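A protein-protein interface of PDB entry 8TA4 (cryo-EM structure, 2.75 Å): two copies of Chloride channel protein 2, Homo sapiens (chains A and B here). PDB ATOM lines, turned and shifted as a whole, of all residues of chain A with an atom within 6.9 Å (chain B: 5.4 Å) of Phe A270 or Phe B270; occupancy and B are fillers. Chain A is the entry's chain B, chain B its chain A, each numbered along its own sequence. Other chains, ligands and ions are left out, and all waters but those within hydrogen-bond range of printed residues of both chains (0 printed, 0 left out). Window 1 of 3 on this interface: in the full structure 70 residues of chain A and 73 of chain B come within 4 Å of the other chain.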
ATOM      1  N   LEU A 171      -1.185   0.641  17.774  1.00  0.00           N
ATOM      2  CA  LEU A 171      -1.061  -0.809  17.666  1.00  0.00           C
ATOM      3  C   LEU A 171      -1.161  -1.315  16.233  1.00  0.00           C
ATOM      4  O   LEU A 171      -0.801  -2.467  15.979  1.00  0.00           O
ATOM      5  CB  LEU A 171      -2.122  -1.496  18.523  1.00  0.00           C
ATOM      6  CG  LEU A 171      -1.835  -1.581  20.020  1.00  0.00           C
ATOM      7  CD1 LEU A 171      -2.953  -2.307  20.729  1.00  0.00           C
ATOM      8  CD2 LEU A 171      -0.516  -2.268  20.271  1.00  0.00           C
ATOM      9  N   THR A 237       2.903  -4.472  19.208  1.00  0.00           N
ATOM     10  CA  THR A 237       1.875  -5.289  19.843  1.00  0.00           C
ATOM     11  C   THR A 237       2.430  -6.029  21.052  1.00  0.00           C
ATOM     12  O   THR A 237       1.841  -5.989  22.140  1.00  0.00           O
ATOM     13  CB  THR A 237       1.292  -6.274  18.828  1.00  0.00           C
ATOM     14  OG1 THR A 237       0.878  -5.564  17.656  1.00  0.00           O
ATOM     15  CG2 THR A 237       0.096  -6.994  19.412  1.00  0.00           C
ATOM     16  N   ALA A 241       0.303  -4.516  24.184  1.00  0.00           N
ATOM     17  CA  ALA A 241      -0.980  -5.162  24.446  1.00  0.00           C
ATOM     18  C   ALA A 241      -1.136  -5.507  25.925  1.00  0.00           C
ATOM     19  O   ALA A 241      -2.180  -5.237  26.541  1.00  0.00           O
ATOM     20  CB  ALA A 241      -1.114  -6.410  23.577  1.00  0.00           C
ATOM     21  N   ALA A 242      -0.098  -6.101  26.516  1.00  0.00           N
ATOM     22  CA  ALA A 242      -0.135  -6.405  27.940  1.00  0.00           C
ATOM     23  C   ALA A 242      -0.265  -5.135  28.766  1.00  0.00           C
ATOM     24  O   ALA A 242      -0.952  -5.121  29.792  1.00  0.00           O
ATOM     25  CB  ALA A 242       1.114  -7.184  28.340  1.00  0.00           C
ATOM     26  N   ALA A 245      -3.889  -4.023  28.748  1.00  0.00           N
ATOM     27  CA  ALA A 245      -4.673  -4.897  29.618  1.00  0.00           C
ATOM     28  C   ALA A 245      -4.464  -4.552  31.088  1.00  0.00           C
ATOM     29  O   ALA A 245      -5.429  -4.455  31.858  1.00  0.00           O
ATOM     30  CB  ALA A 245      -4.316  -6.357  29.356  1.00  0.00           C
ATOM     31  N   VAL A 259      -8.726  -7.300  31.263  1.00  0.00           N
ATOM     32  CA  VAL A 259      -8.007  -7.864  30.121  1.00  0.00           C
ATOM     33  C   VAL A 259      -8.952  -8.047  28.939  1.00  0.00           C
ATOM     34  O   VAL A 259      -8.644  -7.664  27.800  1.00  0.00           O
ATOM     35  CB  VAL A 259      -7.334  -9.190  30.519  1.00  0.00           C
ATOM     36  CG1 VAL A 259      -6.734  -9.867  29.306  1.00  0.00           C
ATOM     37  CG2 VAL A 259      -6.274  -8.949  31.569  1.00  0.00           C
ATOM     38  N   SER A 262      -9.925  -4.674  27.406  1.00  0.00           N
ATOM     39  CA  SER A 262      -8.840  -4.089  26.630  1.00  0.00           C
ATOM     40  C   SER A 262      -8.662  -4.790  25.290  1.00  0.00           C
ATOM     41  O   SER A 262      -8.309  -4.141  24.302  1.00  0.00           O
ATOM     42  CB  SER A 262      -7.541  -4.132  27.427  1.00  0.00           C
ATOM     43  OG  SER A 262      -6.733  -5.217  27.018  1.00  0.00           O
ATOM     44  N   ILE A 263      -8.888  -6.106  25.233  1.00  0.00           N
ATOM     45  CA  ILE A 263      -8.788  -6.804  23.951  1.00  0.00           C
ATOM     46  C   ILE A 263      -9.821  -6.270  22.961  1.00  0.00           C
ATOM     47  O   ILE A 263      -9.537  -6.121  21.766  1.00  0.00           O
ATOM     48  CB  ILE A 263      -8.932  -8.324  24.151  1.00  0.00           C
ATOM     49  CG1 ILE A 263      -7.631  -8.922  24.675  1.00  0.00           C
ATOM     50  CG2 ILE A 263      -9.341  -9.007  22.857  1.00  0.00           C
ATOM     51  CD1 ILE A 263      -7.779 -10.330  25.184  1.00  0.00           C
ATOM     52  N   GLU A 264     -11.031  -5.974  23.436  1.00  0.00           N
ATOM     53  CA  GLU A 264     -12.120  -5.630  22.530  1.00  0.00           C
ATOM     54  C   GLU A 264     -12.008  -4.215  21.977  1.00  0.00           C
ATOM     55  O   GLU A 264     -12.439  -3.963  20.847  1.00  0.00           O
ATOM     56  CB  GLU A 264     -13.462  -5.799  23.237  1.00  0.00           C
ATOM     57  CG  GLU A 264     -13.968  -7.220  23.290  1.00  0.00           C
ATOM     58  CD  GLU A 264     -15.330  -7.319  23.930  1.00  0.00           C
ATOM     59  OE1 GLU A 264     -15.400  -7.402  25.170  1.00  0.00           O
ATOM     60  OE2 GLU A 264     -16.333  -7.314  23.192  1.00  0.00           O
ATOM     61  N   THR A 266      -9.171  -2.184  21.615  1.00  0.00           N
ATOM     62  CA  THR A 266      -7.918  -1.749  21.016  1.00  0.00           C
ATOM     63  C   THR A 266      -7.487  -2.582  19.820  1.00  0.00           C
ATOM     64  O   THR A 266      -6.438  -2.294  19.237  1.00  0.00           O
ATOM     65  CB  THR A 266      -6.796  -1.756  22.062  1.00  0.00           C
ATOM     66  OG1 THR A 266      -6.700  -3.055  22.658  1.00  0.00           O
ATOM     67  CG2 THR A 266      -7.060  -0.720  23.140  1.00  0.00           C
ATOM     68  N   SER A 267      -8.255  -3.592  19.426  1.00  0.00           N
ATOM     69  CA  SER A 267      -7.820  -4.461  18.341  1.00  0.00           C
ATOM     70  C   SER A 267      -9.025  -5.163  17.735  1.00  0.00           C
ATOM     71  O   SER A 267     -10.131  -5.129  18.277  1.00  0.00           O
ATOM     72  CB  SER A 267      -6.787  -5.476  18.827  1.00  0.00           C
ATOM     73  OG  SER A 267      -7.355  -6.368  19.766  1.00  0.00           O
ATOM     74  N   THR A 268      -8.790  -5.788  16.583  1.00  0.00           N
ATOM     75  CA  THR A 268      -9.764  -6.623  15.893  1.00  0.00           C
ATOM     76  C   THR A 268      -9.459  -8.108  16.027  1.00  0.00           C
ATOM     77  O   THR A 268     -10.356  -8.895  16.330  1.00  0.00           O
ATOM     78  CB  THR A 268      -9.820  -6.252  14.408  1.00  0.00           C
ATOM     79  OG1 THR A 268     -10.028  -4.842  14.275  1.00  0.00           O
ATOM     80  CG2 THR A 268     -10.944  -6.987  13.717  1.00  0.00           C
ATOM     81  N   PHE A 269      -8.209  -8.503  15.800  1.00  0.00           N
ATOM     82  CA  PHE A 269      -7.730  -9.853  16.057  1.00  0.00           C
ATOM     83  C   PHE A 269      -6.710  -9.786  17.179  1.00  0.00           C
ATOM     84  O   PHE A 269      -5.761  -8.999  17.110  1.00  0.00           O
ATOM     85  CB  PHE A 269      -7.079 -10.473  14.820  1.00  0.00           C
ATOM     86  CG  PHE A 269      -8.036 -10.796  13.719  1.00  0.00           C
ATOM     87  CD1 PHE A 269      -8.386  -9.839  12.785  1.00  0.00           C
ATOM     88  CD2 PHE A 269      -8.567 -12.062  13.598  1.00  0.00           C
ATOM     89  CE1 PHE A 269      -9.257 -10.136  11.767  1.00  0.00           C
ATOM     90  CE2 PHE A 269      -9.439 -12.363  12.579  1.00  0.00           C
ATOM     91  CZ  PHE A 269      -9.784 -11.399  11.664  1.00  0.00           C
ATOM     92  N   PHE A 270      -6.896 -10.608  18.206  1.00  0.00           N
ATOM     93  CA  PHE A 270      -5.965 -10.671  19.323  1.00  0.00           C
ATOM     94  C   PHE A 270      -5.463 -12.095  19.483  1.00  0.00           C
ATOM     95  O   PHE A 270      -6.262 -13.031  19.574  1.00  0.00           O
ATOM     96  CB  PHE A 270      -6.624 -10.193  20.614  1.00  0.00           C
ATOM     97  CG  PHE A 270      -5.658  -9.633  21.609  1.00  0.00           C
ATOM     98  CD1 PHE A 270      -5.227  -8.326  21.510  1.00  0.00           C
ATOM     99  CD2 PHE A 270      -5.190 -10.409  22.647  1.00  0.00           C
ATOM    100  CE1 PHE A 270      -4.341  -7.808  22.430  1.00  0.00           C
ATOM    101  CE2 PHE A 270      -4.310  -9.895  23.568  1.00  0.00           C
ATOM    102  CZ  PHE A 270      -3.882  -8.597  23.458  1.00  0.00           C
ATOM    103  N   ALA A 271      -4.145 -12.252  19.526  1.00  0.00           N
ATOM    104  CA  ALA A 271      -3.559 -13.568  19.696  1.00  0.00           C
ATOM    105  C   ALA A 271      -3.853 -14.103  21.092  1.00  0.00           C
ATOM    106  O   ALA A 271      -4.219 -13.365  22.007  1.00  0.00           O
ATOM    107  CB  ALA A 271      -2.050 -13.520  19.461  1.00  0.00           C
ATOM    108  N   VAL A 272      -3.709 -15.417  21.241  1.00  0.00           N
ATOM    109  CA  VAL A 272      -3.897 -16.018  22.551  1.00  0.00           C
ATOM    110  C   VAL A 272      -2.656 -15.822  23.417  1.00  0.00           C
ATOM    111  O   VAL A 272      -2.757 -15.763  24.647  1.00  0.00           O
ATOM    112  CB  VAL A 272      -4.274 -17.501  22.393  1.00  0.00           C
ATOM    113  CG1 VAL A 272      -4.530 -18.142  23.737  1.00  0.00           C
ATOM    114  CG2 VAL A 272      -5.508 -17.631  21.526  1.00  0.00           C
ATOM    115  N   ARG A 273      -1.479 -15.693  22.801  1.00  0.00           N
ATOM    116  CA  ARG A 273      -0.256 -15.480  23.568  1.00  0.00           C
ATOM    117  C   ARG A 273      -0.293 -14.155  24.319  1.00  0.00           C
ATOM    118  O   ARG A 273       0.087 -14.083  25.495  1.00  0.00           O
ATOM    119  CB  ARG A 273       0.957 -15.525  22.643  1.00  0.00           C
ATOM    120  CG  ARG A 273       1.710 -16.837  22.662  1.00  0.00           C
ATOM    121  CD  ARG A 273       2.935 -16.795  21.763  1.00  0.00           C
ATOM    122  NE  ARG A 273       3.762 -15.618  21.999  1.00  0.00           N
ATOM    123  CZ  ARG A 273       3.819 -14.565  21.197  1.00  0.00           C
ATOM    124  NH1 ARG A 273       3.092 -14.496  20.095  1.00  0.00           N
ATOM    125  NH2 ARG A 273       4.620 -13.553  21.513  1.00  0.00           N
ATOM    126  N   ASN A 274      -0.733 -13.091  23.652  1.00  0.00           N
ATOM    127  CA  ASN A 274      -0.839 -11.804  24.325  1.00  0.00           C
ATOM    128  C   ASN A 274      -1.940 -11.820  25.375  1.00  0.00           C
ATOM    129  O   ASN A 274      -1.845 -11.110  26.381  1.00  0.00           O
ATOM    130  CB  ASN A 274      -1.071 -10.697  23.300  1.00  0.00           C
ATOM    131  CG  ASN A 274       0.062 -10.582  22.300  1.00  0.00           C
ATOM    132  OD1 ASN A 274       1.215 -10.878  22.609  1.00  0.00           O
ATOM    133  ND2 ASN A 274      -0.265 -10.146  21.090  1.00  0.00           N
ATOM    134  N   TYR A 275      -2.981 -12.627  25.166  1.00  0.00           N
ATOM    135  CA  TYR A 275      -3.984 -12.839  26.203  1.00  0.00           C
ATOM    136  C   TYR A 275      -3.363 -13.471  27.444  1.00  0.00           C
ATOM    137  O   TYR A 275      -3.643 -13.047  28.572  1.00  0.00           O
ATOM    138  CB  TYR A 275      -5.111 -13.706  25.645  1.00  0.00           C
ATOM    139  CG  TYR A 275      -6.167 -14.130  26.635  1.00  0.00           C
ATOM    140  CD1 TYR A 275      -6.766 -13.215  27.486  1.00  0.00           C
ATOM    141  CD2 TYR A 275      -6.582 -15.450  26.702  1.00  0.00           C
ATOM    142  CE1 TYR A 275      -7.738 -13.606  28.380  1.00  0.00           C
ATOM    143  CE2 TYR A 275      -7.550 -15.847  27.592  1.00  0.00           C
ATOM    144  CZ  TYR A 275      -8.125 -14.925  28.429  1.00  0.00           C
ATOM    145  OH  TYR A 275      -9.092 -15.326  29.317  1.00  0.00           O
ATOM    146  N   TRP A 276      -2.495 -14.466  27.253  1.00  0.00           N
ATOM    147  CA  TRP A 276      -1.799 -15.073  28.385  1.00  0.00           C
ATOM    148  C   TRP A 276      -0.904 -14.066  29.096  1.00  0.00           C
ATOM    149  O   TRP A 276      -0.845 -14.038  30.332  1.00  0.00           O
ATOM    150  CB  TRP A 276      -0.968 -16.266  27.920  1.00  0.00           C
ATOM    151  CG  TRP A 276      -1.760 -17.408  27.389  1.00  0.00           C
ATOM    152  CD1 TRP A 276      -3.056 -17.704  27.666  1.00  0.00           C
ATOM    153  CD2 TRP A 276      -1.296 -18.428  26.500  1.00  0.00           C
ATOM    154  NE1 TRP A 276      -3.438 -18.839  26.997  1.00  0.00           N
ATOM    155  CE2 TRP A 276      -2.372 -19.304  26.274  1.00  0.00           C
ATOM    156  CE3 TRP A 276      -0.076 -18.683  25.869  1.00  0.00           C
ATOM    157  CZ2 TRP A 276      -2.267 -20.413  25.445  1.00  0.00           C
ATOM    158  CZ3 TRP A 276       0.025 -19.785  25.046  1.00  0.00           C
ATOM    159  CH2 TRP A 276      -1.063 -20.637  24.841  1.00  0.00           C
ATOM    160  N   GLY A 278      -1.155 -10.727  29.177  1.00  0.00           N
ATOM    161  CA  GLY A 278      -1.988  -9.793  29.912  1.00  0.00           C
ATOM    162  C   GLY A 278      -2.572 -10.403  31.169  1.00  0.00           C
ATOM    163  O   GLY A 278      -2.634  -9.753  32.212  1.00  0.00           O
ATOM    164  N   LEU A 812      -4.821  -7.034  10.142  1.00  0.00           N
ATOM    165  CA  LEU A 812      -3.780  -7.788  10.835  1.00  0.00           C
ATOM    166  C   LEU A 812      -2.378  -7.518  10.307  1.00  0.00           C
ATOM    167  O   LEU A 812      -1.425  -7.461  11.090  1.00  0.00           O
ATOM    168  CB  LEU A 812      -4.060  -9.288  10.747  1.00  0.00           C
ATOM    169  CG  LEU A 812      -4.415 -10.000  12.051  1.00  0.00           C
ATOM    170  CD1 LEU A 812      -4.263 -11.493  11.861  1.00  0.00           C
ATOM    171  CD2 LEU A 812      -3.559  -9.507  13.210  1.00  0.00           C
ATOM    172  N   ALA B 241     -16.929 -21.650  14.247  1.00  0.00           N
ATOM    173  CA  ALA B 241     -16.438 -21.079  15.495  1.00  0.00           C
ATOM    174  C   ALA B 241     -17.578 -20.803  16.464  1.00  0.00           C
ATOM    175  O   ALA B 241     -17.474 -21.112  17.665  1.00  0.00           O
ATOM    176  CB  ALA B 241     -15.655 -19.801  15.203  1.00  0.00           C
ATOM    177  N   ILE B 263     -12.440 -20.484  22.289  1.00  0.00           N
ATOM    178  CA  ILE B 263     -11.547 -19.622  21.516  1.00  0.00           C
ATOM    179  C   ILE B 263     -10.099 -20.069  21.671  1.00  0.00           C
ATOM    180  O   ILE B 263      -9.345 -20.130  20.694  1.00  0.00           O
ATOM    181  CB  ILE B 263     -11.728 -18.148  21.921  1.00  0.00           C
ATOM    182  CG1 ILE B 263     -12.951 -17.551  21.237  1.00  0.00           C
ATOM    183  CG2 ILE B 263     -10.503 -17.341  21.565  1.00  0.00           C
ATOM    184  CD1 ILE B 263     -13.507 -16.345  21.945  1.00  0.00           C
ATOM    185  N   SER B 267      -8.127 -22.096  17.938  1.00  0.00           N
ATOM    186  CA  SER B 267      -7.554 -21.079  17.068  1.00  0.00           C
ATOM    187  C   SER B 267      -6.399 -20.393  17.778  1.00  0.00           C
ATOM    188  O   SER B 267      -6.108 -20.660  18.945  1.00  0.00           O
ATOM    189  CB  SER B 267      -8.606 -20.052  16.642  1.00  0.00           C
ATOM    190  OG  SER B 267      -9.180 -19.413  17.767  1.00  0.00           O
ATOM    191  N   THR B 268      -5.730 -19.512  17.039  1.00  0.00           N
ATOM    192  CA  THR B 268      -4.711 -18.616  17.571  1.00  0.00           C
ATOM    193  C   THR B 268      -5.130 -17.158  17.530  1.00  0.00           C
ATOM    194  O   THR B 268      -4.964 -16.444  18.517  1.00  0.00           O
ATOM    195  CB  THR B 268      -3.401 -18.780  16.795  1.00  0.00           C
ATOM    196  OG1 THR B 268      -3.015 -20.158  16.792  1.00  0.00           O
ATOM    197  CG2 THR B 268      -2.304 -17.960  17.431  1.00  0.00           C
ATOM    198  N   PHE B 269      -5.674 -16.699  16.407  1.00  0.00           N
ATOM    199  CA  PHE B 269      -6.224 -15.360  16.275  1.00  0.00           C
ATOM    200  C   PHE B 269      -7.729 -15.483  16.109  1.00  0.00           C
ATOM    201  O   PHE B 269      -8.199 -16.193  15.215  1.00  0.00           O
ATOM    202  CB  PHE B 269      -5.626 -14.624  15.075  1.00  0.00           C
ATOM    203  CG  PHE B 269      -4.208 -14.190  15.269  1.00  0.00           C
ATOM    204  CD1 PHE B 269      -3.165 -15.038  14.958  1.00  0.00           C
ATOM    205  CD2 PHE B 269      -3.916 -12.929  15.741  1.00  0.00           C
ATOM    206  CE1 PHE B 269      -1.861 -14.640  15.132  1.00  0.00           C
ATOM    207  CE2 PHE B 269      -2.613 -12.527  15.914  1.00  0.00           C
ATOM    208  CZ  PHE B 269      -1.585 -13.383  15.608  1.00  0.00           C
ATOM    209  N   PHE B 270      -8.481 -14.799  16.964  1.00  0.00           N
ATOM    210  CA  PHE B 270      -9.935 -14.843  16.909  1.00  0.00           C
ATOM    211  C   PHE B 270     -10.481 -13.431  16.794  1.00  0.00           C
ATOM    212  O   PHE B 270     -10.076 -12.541  17.548  1.00  0.00           O
ATOM    213  CB  PHE B 270     -10.512 -15.532  18.143  1.00  0.00           C
ATOM    214  CG  PHE B 270     -11.840 -16.177  17.909  1.00  0.00           C
ATOM    215  CD1 PHE B 270     -11.932 -17.372  17.226  1.00  0.00           C
ATOM    216  CD2 PHE B 270     -12.998 -15.593  18.378  1.00  0.00           C
ATOM    217  CE1 PHE B 270     -13.153 -17.968  17.016  1.00  0.00           C
ATOM    218  CE2 PHE B 270     -14.220 -16.189  18.175  1.00  0.00           C
ATOM    219  CZ  PHE B 270     -14.299 -17.377  17.492  1.00  0.00           C
ATOM    220  N   ALA B 271     -11.395 -13.230  15.852  1.00  0.00           N
ATOM    221  CA  ALA B 271     -12.007 -11.924  15.682  1.00  0.00           C
ATOM    222  C   ALA B 271     -12.951 -11.627  16.838  1.00  0.00           C
ATOM    223  O   ALA B 271     -13.492 -12.530  17.477  1.00  0.00           O
ATOM    224  CB  ALA B 271     -12.762 -11.855  14.357  1.00  0.00           C
ATOM    225  N   VAL B 272     -13.129 -10.337  17.117  1.00  0.00           N
ATOM    226  CA  VAL B 272     -14.070  -9.934  18.152  1.00  0.00           C
ATOM    227  C   VAL B 272     -15.506 -10.177  17.699  1.00  0.00           C
ATOM    228  O   VAL B 272     -16.390 -10.433  18.526  1.00  0.00           O
ATOM    229  CB  VAL B 272     -13.821  -8.465  18.537  1.00  0.00           C
ATOM    230  CG1 VAL B 272     -14.636  -8.085  19.748  1.00  0.00           C
ATOM    231  CG2 VAL B 272     -12.350  -8.248  18.823  1.00  0.00           C
ATOM    232  N   ASN B 274     -16.715 -12.749  15.922  1.00  0.00           N
ATOM    233  CA  ASN B 274     -17.091 -14.125  16.209  1.00  0.00           C
ATOM    234  C   ASN B 274     -17.250 -14.355  17.707  1.00  0.00           C
ATOM    235  O   ASN B 274     -18.068 -15.183  18.122  1.00  0.00           O
ATOM    236  CB  ASN B 274     -16.063 -15.078  15.607  1.00  0.00           C
ATOM    237  CG  ASN B 274     -16.066 -15.056  14.092  1.00  0.00           C
ATOM    238  OD1 ASN B 274     -17.061 -14.696  13.468  1.00  0.00           O
ATOM    239  ND2 ASN B 274     -14.946 -15.438  13.496  1.00  0.00           N
ATOM    240  N   TYR B 275     -16.488 -13.630  18.527  1.00  0.00           N
ATOM    241  CA  TYR B 275     -16.694 -13.667  19.972  1.00  0.00           C
ATOM    242  C   TYR B 275     -18.085 -13.161  20.340  1.00  0.00           C
ATOM    243  O   TYR B 275     -18.770 -13.761  21.177  1.00  0.00           O
ATOM    244  CB  TYR B 275     -15.602 -12.847  20.658  1.00  0.00           C
ATOM    245  CG  TYR B 275     -15.766 -12.635  22.147  1.00  0.00           C
ATOM    246  CD1 TYR B 275     -16.119 -13.678  22.989  1.00  0.00           C
ATOM    247  CD2 TYR B 275     -15.535 -11.390  22.711  1.00  0.00           C
ATOM    248  CE1 TYR B 275     -16.256 -13.480  24.346  1.00  0.00           C
ATOM    249  CE2 TYR B 275     -15.668 -11.183  24.064  1.00  0.00           C
ATOM    250  CZ  TYR B 275     -16.027 -12.229  24.878  1.00  0.00           C
ATOM    251  OH  TYR B 275     -16.161 -12.022  26.230  1.00  0.00           O
ATOM    252  N   LEU B 812      -3.368 -17.634  10.184  1.00  0.00           N
ATOM    253  CA  LEU B 812      -4.685 -17.068   9.926  1.00  0.00           C
ATOM    254  C   LEU B 812      -4.982 -16.766   8.464  1.00  0.00           C
ATOM    255  O   LEU B 812      -6.151 -16.564   8.126  1.00  0.00           O
ATOM    256  CB  LEU B 812      -4.884 -15.783  10.742  1.00  0.00           C
ATOM    257  CG  LEU B 812      -6.348 -15.527  11.108  1.00  0.00           C
ATOM    258  CD1 LEU B 812      -6.809 -16.453  12.222  1.00  0.00           C
ATOM    259  CD2 LEU B 812      -6.560 -14.087  11.492  1.00  0.00           C
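Ser A267 touches Val B272, but with the chains exchanged Val A272 does not touch Ser B267 (4.02 Å).
Phe A269 touches Leu B812, but with the chains exchanged Leu A812 does not touch Phe B269 (4.2 Å).
Phe A270 touches its own counterpart, Phe B270.
Leu A812 touches its own counterpart, Leu B812.
Positions printed for both chains: 241, 263, 267, 268, 269, 270, 271, 272, 274, 275 and 812.
Of chain B, only Thr B268 and Phe B270 come within 4 Å of Phe A270.
Phe B270 touches just these residues of chain A: Thr A268, Phe A269 and Phe A270.
Printed residues of chain A within 4 Å of Thr B268: Phe A270 (3.8 Å), Ala A271 (3.4 Å) and Val A272 (3.2 Å).
Printed residues of chain A within 4 Å of Phe B269: Ala A271 (3.7 Å).
Printed residues of chain B within 4 Å of Glu A264: Val B272 and Tyr B275.
Ala A242 touches none of the printed residues of chain B.
Printed residues of chain A that touch a printed residue of chain B: Glu A264, Ser A267, Thr A268, Phe A269, Phe A270, Ala A271, Val A272 and Leu A812.
Hydrophobic or aromatic side chains of chain A within 4 Å of the printed part of chain B: Phe A269, Ala A271, Val A272 and Leu A812.
Among the printed residues, 15 pairs touch across the chains.
Among the printed residues, no Asp or Glu carboxylate lies within 4 Å of a Lys or Arg side-chain nitrogen of the other chain.
O of Ile A263 is in hydrogen-bond range of OG of Ser A267 (3.0 Å).
Among the printed residues, pairs that only touch across the chains: Ala A271 with Thr B268 (3.4 Å), Leu A812 with Leu B812 (3.5 Å), Thr A268 with Ala B271 (3.5 Å), Phe A269 with Leu B812 (3.5 Å), Glu A264 with Val B272 (3.7 Å), Ala A271 with Phe B269 (3.7 Å), Phe A270 with Phe B270 (3.8 Å), Phe A269 with Ala B271 (3.8 Å), Phe A270 with Thr B268 (3.8 Å), Thr A268 with Phe B270 (3.9 Å), Ser A267 with Val B272 (3.9 Å), Phe A269 with Phe B270 (3.9 Å) and Glu A264 with Tyr B275 (3.9 Å).
O of Thr B268 lies within hydrogen-bond range of N of Val A272 (3.2 Å).
N of Val B272 lies within hydrogen-bond range of O of Thr A268.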
